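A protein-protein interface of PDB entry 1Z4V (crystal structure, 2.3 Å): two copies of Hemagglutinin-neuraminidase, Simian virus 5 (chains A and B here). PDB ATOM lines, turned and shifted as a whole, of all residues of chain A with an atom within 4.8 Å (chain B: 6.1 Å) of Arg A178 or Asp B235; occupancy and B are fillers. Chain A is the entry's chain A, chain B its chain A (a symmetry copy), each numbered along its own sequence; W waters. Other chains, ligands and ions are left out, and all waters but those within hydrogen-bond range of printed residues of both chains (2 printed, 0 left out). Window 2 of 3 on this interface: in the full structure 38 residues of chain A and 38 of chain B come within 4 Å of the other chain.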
ATOM      1  N   TRP A 141     -27.546  20.919  27.151  1.00  0.00           N
ATOM      2  CA  TRP A 141     -28.790  21.525  27.619  1.00  0.00           C
ATOM      3  C   TRP A 141     -29.154  21.050  29.025  1.00  0.00           C
ATOM      4  O   TRP A 141     -28.762  19.968  29.451  1.00  0.00           O
ATOM      5  CB  TRP A 141     -29.944  21.199  26.662  1.00  0.00           C
ATOM      6  CG  TRP A 141     -30.185  19.717  26.427  1.00  0.00           C
ATOM      7  CD1 TRP A 141     -29.777  18.989  25.353  1.00  0.00           C
ATOM      8  CD2 TRP A 141     -30.916  18.800  27.273  1.00  0.00           C
ATOM      9  NE1 TRP A 141     -30.207  17.688  25.469  1.00  0.00           N
ATOM     10  CE2 TRP A 141     -30.906  17.546  26.631  1.00  0.00           C
ATOM     11  CE3 TRP A 141     -31.579  18.926  28.499  1.00  0.00           C
ATOM     12  CZ2 TRP A 141     -31.541  16.409  27.179  1.00  0.00           C
ATOM     13  CZ3 TRP A 141     -32.217  17.788  29.053  1.00  0.00           C
ATOM     14  CH2 TRP A 141     -32.192  16.557  28.392  1.00  0.00           C
ATOM     15  N   MET A 164     -30.285  16.662  32.128  1.00  0.00           N
ATOM     16  CA  MET A 164     -29.279  17.330  31.310  1.00  0.00           C
ATOM     17  C   MET A 164     -28.801  16.353  30.250  1.00  0.00           C
ATOM     18  O   MET A 164     -28.808  15.138  30.459  1.00  0.00           O
ATOM     19  CB  MET A 164     -28.113  17.836  32.166  1.00  0.00           C
ATOM     20  CG  MET A 164     -27.288  16.766  32.860  1.00  0.00           C
ATOM     21  SD  MET A 164     -25.984  17.546  33.897  1.00  0.00           S
ATOM     22  CE  MET A 164     -26.981  18.087  35.275  1.00  0.00           C
ATOM     23  N   GLY A 165     -28.415  16.889  29.099  1.00  0.00           N
ATOM     24  CA  GLY A 165     -27.952  16.050  28.016  1.00  0.00           C
ATOM     25  C   GLY A 165     -27.432  16.844  26.838  1.00  0.00           C
ATOM     26  O   GLY A 165     -27.112  18.035  26.960  1.00  0.00           O
ATOM     27  N   ILE A 166     -27.358  16.190  25.686  1.00  0.00           N
ATOM     28  CA  ILE A 166     -26.852  16.811  24.474  1.00  0.00           C
ATOM     29  C   ILE A 166     -27.809  16.607  23.310  1.00  0.00           C
ATOM     30  O   ILE A 166     -28.804  15.893  23.432  1.00  0.00           O
ATOM     31  CB  ILE A 166     -25.500  16.182  24.085  1.00  0.00           C
ATOM     32  CG1 ILE A 166     -25.717  14.697  23.766  1.00  0.00           C
ATOM     33  CG2 ILE A 166     -24.503  16.355  25.214  1.00  0.00           C
ATOM     34  CD1 ILE A 166     -24.489  13.963  23.330  1.00  0.00           C
ATOM     35  N   GLU A 168     -28.174  15.400  19.240  1.00  0.00           N
ATOM     36  CA  GLU A 168     -27.497  14.644  18.197  1.00  0.00           C
ATOM     37  C   GLU A 168     -28.487  14.361  17.084  1.00  0.00           C
ATOM     38  O   GLU A 168     -29.687  14.230  17.320  1.00  0.00           O
ATOM     39  CB  GLU A 168     -26.921  13.329  18.746  1.00  0.00           C
ATOM     40  CG  GLU A 168     -27.946  12.291  19.144  1.00  0.00           C
ATOM     41  CD  GLU A 168     -27.297  11.002  19.643  1.00  0.00           C
ATOM     42  OE1 GLU A 168     -26.122  11.057  20.102  1.00  0.00           O
ATOM     43  OE2 GLU A 168     -27.962   9.936  19.596  1.00  0.00           O
ATOM     44  N   PHE A 176     -32.371  14.853  18.277  1.00  0.00           N
ATOM     45  CA  PHE A 176     -32.782  13.935  19.313  1.00  0.00           C
ATOM     46  C   PHE A 176     -32.088  14.478  20.547  1.00  0.00           C
ATOM     47  O   PHE A 176     -30.865  14.567  20.571  1.00  0.00           O
ATOM     48  CB  PHE A 176     -32.286  12.516  19.049  1.00  0.00           C
ATOM     49  CG  PHE A 176     -32.239  11.646  20.292  1.00  0.00           C
ATOM     50  CD1 PHE A 176     -33.351  11.534  21.127  1.00  0.00           C
ATOM     51  CD2 PHE A 176     -31.084  10.950  20.625  1.00  0.00           C
ATOM     52  CE1 PHE A 176     -33.316  10.738  22.274  1.00  0.00           C
ATOM     53  CE2 PHE A 176     -31.032  10.148  21.769  1.00  0.00           C
ATOM     54  CZ  PHE A 176     -32.156  10.042  22.601  1.00  0.00           C
ATOM     55  N   PHE A 177     -32.858  14.884  21.550  1.00  0.00           N
ATOM     56  CA  PHE A 177     -32.269  15.390  22.782  1.00  0.00           C
ATOM     57  C   PHE A 177     -31.943  14.189  23.646  1.00  0.00           C
ATOM     58  O   PHE A 177     -32.822  13.598  24.269  1.00  0.00           O
ATOM     59  CB  PHE A 177     -33.244  16.322  23.487  1.00  0.00           C
ATOM     60  CG  PHE A 177     -33.348  17.657  22.835  1.00  0.00           C
ATOM     61  CD1 PHE A 177     -33.864  17.777  21.551  1.00  0.00           C
ATOM     62  CD2 PHE A 177     -32.877  18.790  23.470  1.00  0.00           C
ATOM     63  CE1 PHE A 177     -33.903  19.013  20.904  1.00  0.00           C
ATOM     64  CE2 PHE A 177     -32.910  20.034  22.828  1.00  0.00           C
ATOM     65  CZ  PHE A 177     -33.428  20.138  21.540  1.00  0.00           C
ATOM     66  N   ARG A 178     -30.665  13.828  23.654  1.00  0.00           N
ATOM     67  CA  ARG A 178     -30.175  12.693  24.406  1.00  0.00           C
ATOM     68  C   ARG A 178     -29.895  13.044  25.871  1.00  0.00           C
ATOM     69  O   ARG A 178     -29.009  13.844  26.178  1.00  0.00           O
ATOM     70  CB  ARG A 178     -28.894  12.173  23.757  1.00  0.00           C
ATOM     71  CG  ARG A 178     -28.444  10.853  24.317  1.00  0.00           C
ATOM     72  CD  ARG A 178     -27.101  10.433  23.783  1.00  0.00           C
ATOM     73  NE  ARG A 178     -26.737   9.157  24.370  1.00  0.00           N
ATOM     74  CZ  ARG A 178     -25.506   8.664  24.398  1.00  0.00           C
ATOM     75  NH1 ARG A 178     -24.506   9.344  23.864  1.00  0.00           N
ATOM     76  NH2 ARG A 178     -25.279   7.500  24.980  1.00  0.00           N
ATOM     77  N   THR A 179     -30.655  12.431  26.769  1.00  0.00           N
ATOM     78  CA  THR A 179     -30.488  12.657  28.192  1.00  0.00           C
ATOM     79  C   THR A 179     -29.289  11.859  28.672  1.00  0.00           C
ATOM     80  O   THR A 179     -29.198  10.654  28.413  1.00  0.00           O
ATOM     81  CB  THR A 179     -31.726  12.175  28.953  1.00  0.00           C
ATOM     82  OG1 THR A 179     -32.873  12.925  28.517  1.00  0.00           O
ATOM     83  CG2 THR A 179     -31.538  12.348  30.471  1.00  0.00           C
ATOM     84  N   LEU A 180     -28.366  12.517  29.366  1.00  0.00           N
ATOM     85  CA  LEU A 180     -27.182  11.833  29.882  1.00  0.00           C
ATOM     86  C   LEU A 180     -27.179  11.748  31.414  1.00  0.00           C
ATOM     87  O   LEU A 180     -26.337  11.073  32.003  1.00  0.00           O
ATOM     88  CB  LEU A 180     -25.912  12.534  29.397  1.00  0.00           C
ATOM     89  CG  LEU A 180     -25.652  12.460  27.892  1.00  0.00           C
ATOM     90  CD1 LEU A 180     -24.253  13.001  27.592  1.00  0.00           C
ATOM     91  CD2 LEU A 180     -25.751  11.020  27.440  1.00  0.00           C
ATOM     92  N   LYS B 181     -28.485   7.066  31.518  1.00  0.00           N
ATOM     93  CA  LYS B 181     -28.027   7.047  30.142  1.00  0.00           C
ATOM     94  C   LYS B 181     -29.183   6.746  29.204  1.00  0.00           C
ATOM     95  O   LYS B 181     -30.041   5.942  29.496  1.00  0.00           O
ATOM     96  CB  LYS B 181     -26.931   6.000  29.901  1.00  0.00           C
ATOM     97  CG  LYS B 181     -26.307   6.147  28.508  1.00  0.00           C
ATOM     98  CD  LYS B 181     -25.383   4.983  28.105  1.00  0.00           C
ATOM     99  CE  LYS B 181     -24.246   4.773  29.098  1.00  0.00           C
ATOM    100  NZ  LYS B 181     -23.427   6.003  29.239  1.00  0.00           N
ATOM    101  N   THR B 182     -29.160   7.397  28.057  1.00  0.00           N
ATOM    102  CA  THR B 182     -30.182   7.239  27.043  1.00  0.00           C
ATOM    103  C   THR B 182     -29.432   6.993  25.719  1.00  0.00           C
ATOM    104  O   THR B 182     -28.318   7.449  25.557  1.00  0.00           O
ATOM    105  CB  THR B 182     -31.012   8.539  27.034  1.00  0.00           C
ATOM    106  OG1 THR B 182     -32.264   8.310  27.704  1.00  0.00           O
ATOM    107  CG2 THR B 182     -31.202   9.070  25.683  1.00  0.00           C
ATOM    108  N   LEU B 183     -30.028   6.233  24.804  1.00  0.00           N
ATOM    109  CA  LEU B 183     -29.454   5.940  23.490  1.00  0.00           C
ATOM    110  C   LEU B 183     -30.600   5.847  22.507  1.00  0.00           C
ATOM    111  O   LEU B 183     -31.687   5.424  22.862  1.00  0.00           O
ATOM    112  CB  LEU B 183     -28.715   4.589  23.449  1.00  0.00           C
ATOM    113  CG  LEU B 183     -27.528   4.336  24.376  1.00  0.00           C
ATOM    114  CD1 LEU B 183     -28.013   3.711  25.679  1.00  0.00           C
ATOM    115  CD2 LEU B 183     -26.569   3.392  23.688  1.00  0.00           C
ATOM    116  N   TYR B 184     -30.354   6.237  21.268  1.00  0.00           N
ATOM    117  CA  TYR B 184     -31.387   6.177  20.247  1.00  0.00           C
ATOM    118  C   TYR B 184     -30.753   5.596  18.994  1.00  0.00           C
ATOM    119  O   TYR B 184     -30.066   6.298  18.258  1.00  0.00           O
ATOM    120  CB  TYR B 184     -31.950   7.578  19.981  1.00  0.00           C
ATOM    121  CG  TYR B 184     -33.231   7.623  19.163  1.00  0.00           C
ATOM    122  CD1 TYR B 184     -34.286   6.741  19.415  1.00  0.00           C
ATOM    123  CD2 TYR B 184     -33.405   8.591  18.164  1.00  0.00           C
ATOM    124  CE1 TYR B 184     -35.495   6.822  18.707  1.00  0.00           C
ATOM    125  CE2 TYR B 184     -34.610   8.683  17.437  1.00  0.00           C
ATOM    126  CZ  TYR B 184     -35.651   7.800  17.714  1.00  0.00           C
ATOM    127  OH  TYR B 184     -36.839   7.912  17.013  1.00  0.00           O
ATOM    128  N   TYR B 232     -22.629  -0.726  27.054  1.00  0.00           N
ATOM    129  CA  TYR B 232     -22.045  -0.580  28.382  1.00  0.00           C
ATOM    130  C   TYR B 232     -22.295   0.799  28.941  1.00  0.00           C
ATOM    131  O   TYR B 232     -22.388   1.780  28.198  1.00  0.00           O
ATOM    132  CB  TYR B 232     -20.539  -0.849  28.334  1.00  0.00           C
ATOM    133  CG  TYR B 232     -20.206  -2.269  27.976  1.00  0.00           C
ATOM    134  CD1 TYR B 232     -20.350  -3.300  28.905  1.00  0.00           C
ATOM    135  CD2 TYR B 232     -19.769  -2.593  26.696  1.00  0.00           C
ATOM    136  CE1 TYR B 232     -20.054  -4.630  28.556  1.00  0.00           C
ATOM    137  CE2 TYR B 232     -19.479  -3.905  26.338  1.00  0.00           C
ATOM    138  CZ  TYR B 232     -19.621  -4.916  27.266  1.00  0.00           C
ATOM    139  OH  TYR B 232     -19.340  -6.212  26.885  1.00  0.00           O
ATOM    140  N   TYR B 233     -22.392   0.865  30.260  1.00  0.00           N
ATOM    141  CA  TYR B 233     -22.647   2.118  30.943  1.00  0.00           C
ATOM    142  C   TYR B 233     -21.558   3.152  30.655  1.00  0.00           C
ATOM    143  O   TYR B 233     -21.755   4.352  30.837  1.00  0.00           O
ATOM    144  CB  TYR B 233     -22.732   1.861  32.450  1.00  0.00           C
ATOM    145  CG  TYR B 233     -23.006   3.100  33.255  1.00  0.00           C
ATOM    146  CD1 TYR B 233     -24.252   3.754  33.188  1.00  0.00           C
ATOM    147  CD2 TYR B 233     -22.025   3.625  34.101  1.00  0.00           C
ATOM    148  CE1 TYR B 233     -24.499   4.883  33.947  1.00  0.00           C
ATOM    149  CE2 TYR B 233     -22.266   4.761  34.861  1.00  0.00           C
ATOM    150  CZ  TYR B 233     -23.495   5.376  34.782  1.00  0.00           C
ATOM    151  OH  TYR B 233     -23.712   6.483  35.555  1.00  0.00           O
ATOM    152  N   ASN B 234     -20.387   2.670  30.214  1.00  0.00           N
ATOM    153  CA  ASN B 234     -19.249   3.544  29.873  1.00  0.00           C
ATOM    154  C   ASN B 234     -19.339   4.060  28.438  1.00  0.00           C
ATOM    155  O   ASN B 234     -18.367   4.579  27.891  1.00  0.00           O
ATOM    156  CB  ASN B 234     -17.881   2.854  30.094  1.00  0.00           C
ATOM    157  CG  ASN B 234     -17.635   1.678  29.166  1.00  0.00           C
ATOM    158  OD1 ASN B 234     -18.233   1.582  28.091  1.00  0.00           O
ATOM    159  ND2 ASN B 234     -16.728   0.793  29.590  1.00  0.00           N
ATOM    160  N   ASP B 235     -20.529   3.938  27.851  1.00  0.00           N
ATOM    161  CA  ASP B 235     -20.798   4.384  26.497  1.00  0.00           C
ATOM    162  C   ASP B 235     -20.187   3.621  25.327  1.00  0.00           C
ATOM    163  O   ASP B 235     -20.327   4.038  24.190  1.00  0.00           O
ATOM    164  CB  ASP B 235     -20.506   5.886  26.364  1.00  0.00           C
ATOM    165  CG  ASP B 235     -21.759   6.683  25.955  1.00  0.00           C
ATOM    166  OD1 ASP B 235     -22.793   6.547  26.645  1.00  0.00           O
ATOM    167  OD2 ASP B 235     -21.725   7.433  24.947  1.00  0.00           O
ATOM    168  N   THR B 236     -19.509   2.513  25.593  1.00  0.00           N
ATOM    169  CA  THR B 236     -18.986   1.700  24.504  1.00  0.00           C
ATOM    170  C   THR B 236     -20.186   0.901  23.976  1.00  0.00           C
ATOM    171  O   THR B 236     -20.999   0.415  24.755  1.00  0.00           O
ATOM    172  CB  THR B 236     -17.961   0.662  24.999  1.00  0.00           C
ATOM    173  OG1 THR B 236     -16.744   1.312  25.362  1.00  0.00           O
ATOM    174  CG2 THR B 236     -17.658  -0.353  23.921  1.00  0.00           C
ATOM    175  N   ILE B 237     -20.304   0.787  22.659  1.00  0.00           N
ATOM    176  CA  ILE B 237     -21.388   0.032  22.045  1.00  0.00           C
ATOM    177  C   ILE B 237     -20.816  -0.956  21.035  1.00  0.00           C
ATOM    178  O   ILE B 237     -20.018  -0.586  20.168  1.00  0.00           O
ATOM    179  CB  ILE B 237     -22.371   0.934  21.295  1.00  0.00           C
ATOM    180  CG1 ILE B 237     -22.962   1.969  22.252  1.00  0.00           C
ATOM    181  CG2 ILE B 237     -23.486   0.096  20.696  1.00  0.00           C
ATOM    182  CD1 ILE B 237     -23.907   2.919  21.572  1.00  0.00           C
HETATM  183  O   HOH W   1     -29.248   8.947  17.388  1.00  0.00           O
HETATM  184  O   HOH W   2     -27.684   7.639  20.898  1.00  0.00           O
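NE of Arg A178 lies within hydrogen-bond range of O of Thr B182 (2.6 Å). The side-chain carboxylate (OD1) of Asp B235 is in salt-bridge range of the guanidinium group (NH2) of Arg A178 (3.1 Å). N of Thr B182 sits close to O of Thr A179, 3.3 Å away.
O of Ile A166 lies within hydrogen-bond range of N of Arg A178. O of Glu A168 sits at hydrogen-bond distance from N of Phe A176, at 2.9 Å. The backbone carbonyl oxygen of Tyr B233 is in hydrogen-bond range of the side-chain amino group of Lys B181, at 2.8 Å. The side-chain carboxylate (OD1) of Asp B235 is in salt-bridge range of the side-chain amino group (NZ) of Lys B181, 2.7 Å away.
Among the printed residues, merely in contact across the chains: Phe A176 with Tyr B184, Phe A176 with Thr B182, Arg A178 with Lys B181, Arg A178 with Leu B183 and Thr A179 with Lys B181.
Arg A178 touches just these residues of chain B: Lys B181, Thr B182, Leu B183 and Asp B235. Of the printed residues of chain A, Asp B235 touches Arg A178. Of the printed residues of chain B, Thr A179 touches Lys B181 and Thr B182. Of the printed residues of chain A, Tyr B184 touches Phe A176. Leu A180 touches none of the printed residues of chain B. Thr B236 touches none of the printed residues of chain A. The nearest residue of chain B that does not touch Arg A178 is Tyr B184 (5.6 Å). The nearest printed residue of chain A that does not touch Asp B235 is Leu A180 (5.4 Å).
Hydrophobic or aromatic side chains of chain B that line the printed part of chain A: Leu B183 and Tyr B184. Hydrophobic or aromatic side chains of chain A within 4 Å of the printed part of chain B: Phe A176. Among the printed residues, 8 pairs touch across the chains. Among the printed residues, Asp or Glu carboxylates within 4 Å of a Lys or Arg side-chain nitrogen of the other chain: Arg A178 with Asp B235 (3.1 Å).
No position is printed for both chains.
Water W2 bridges the side-chain carboxylate (OE2) of Glu A168 (2.7 Å) and the backbone NH (N) of Tyr B184 (3.0 Å). Water W1 lies within hydrogen-bond range of OE2 of Glu A168 (2.7 Å) and O of Tyr B184 (2.9 Å).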
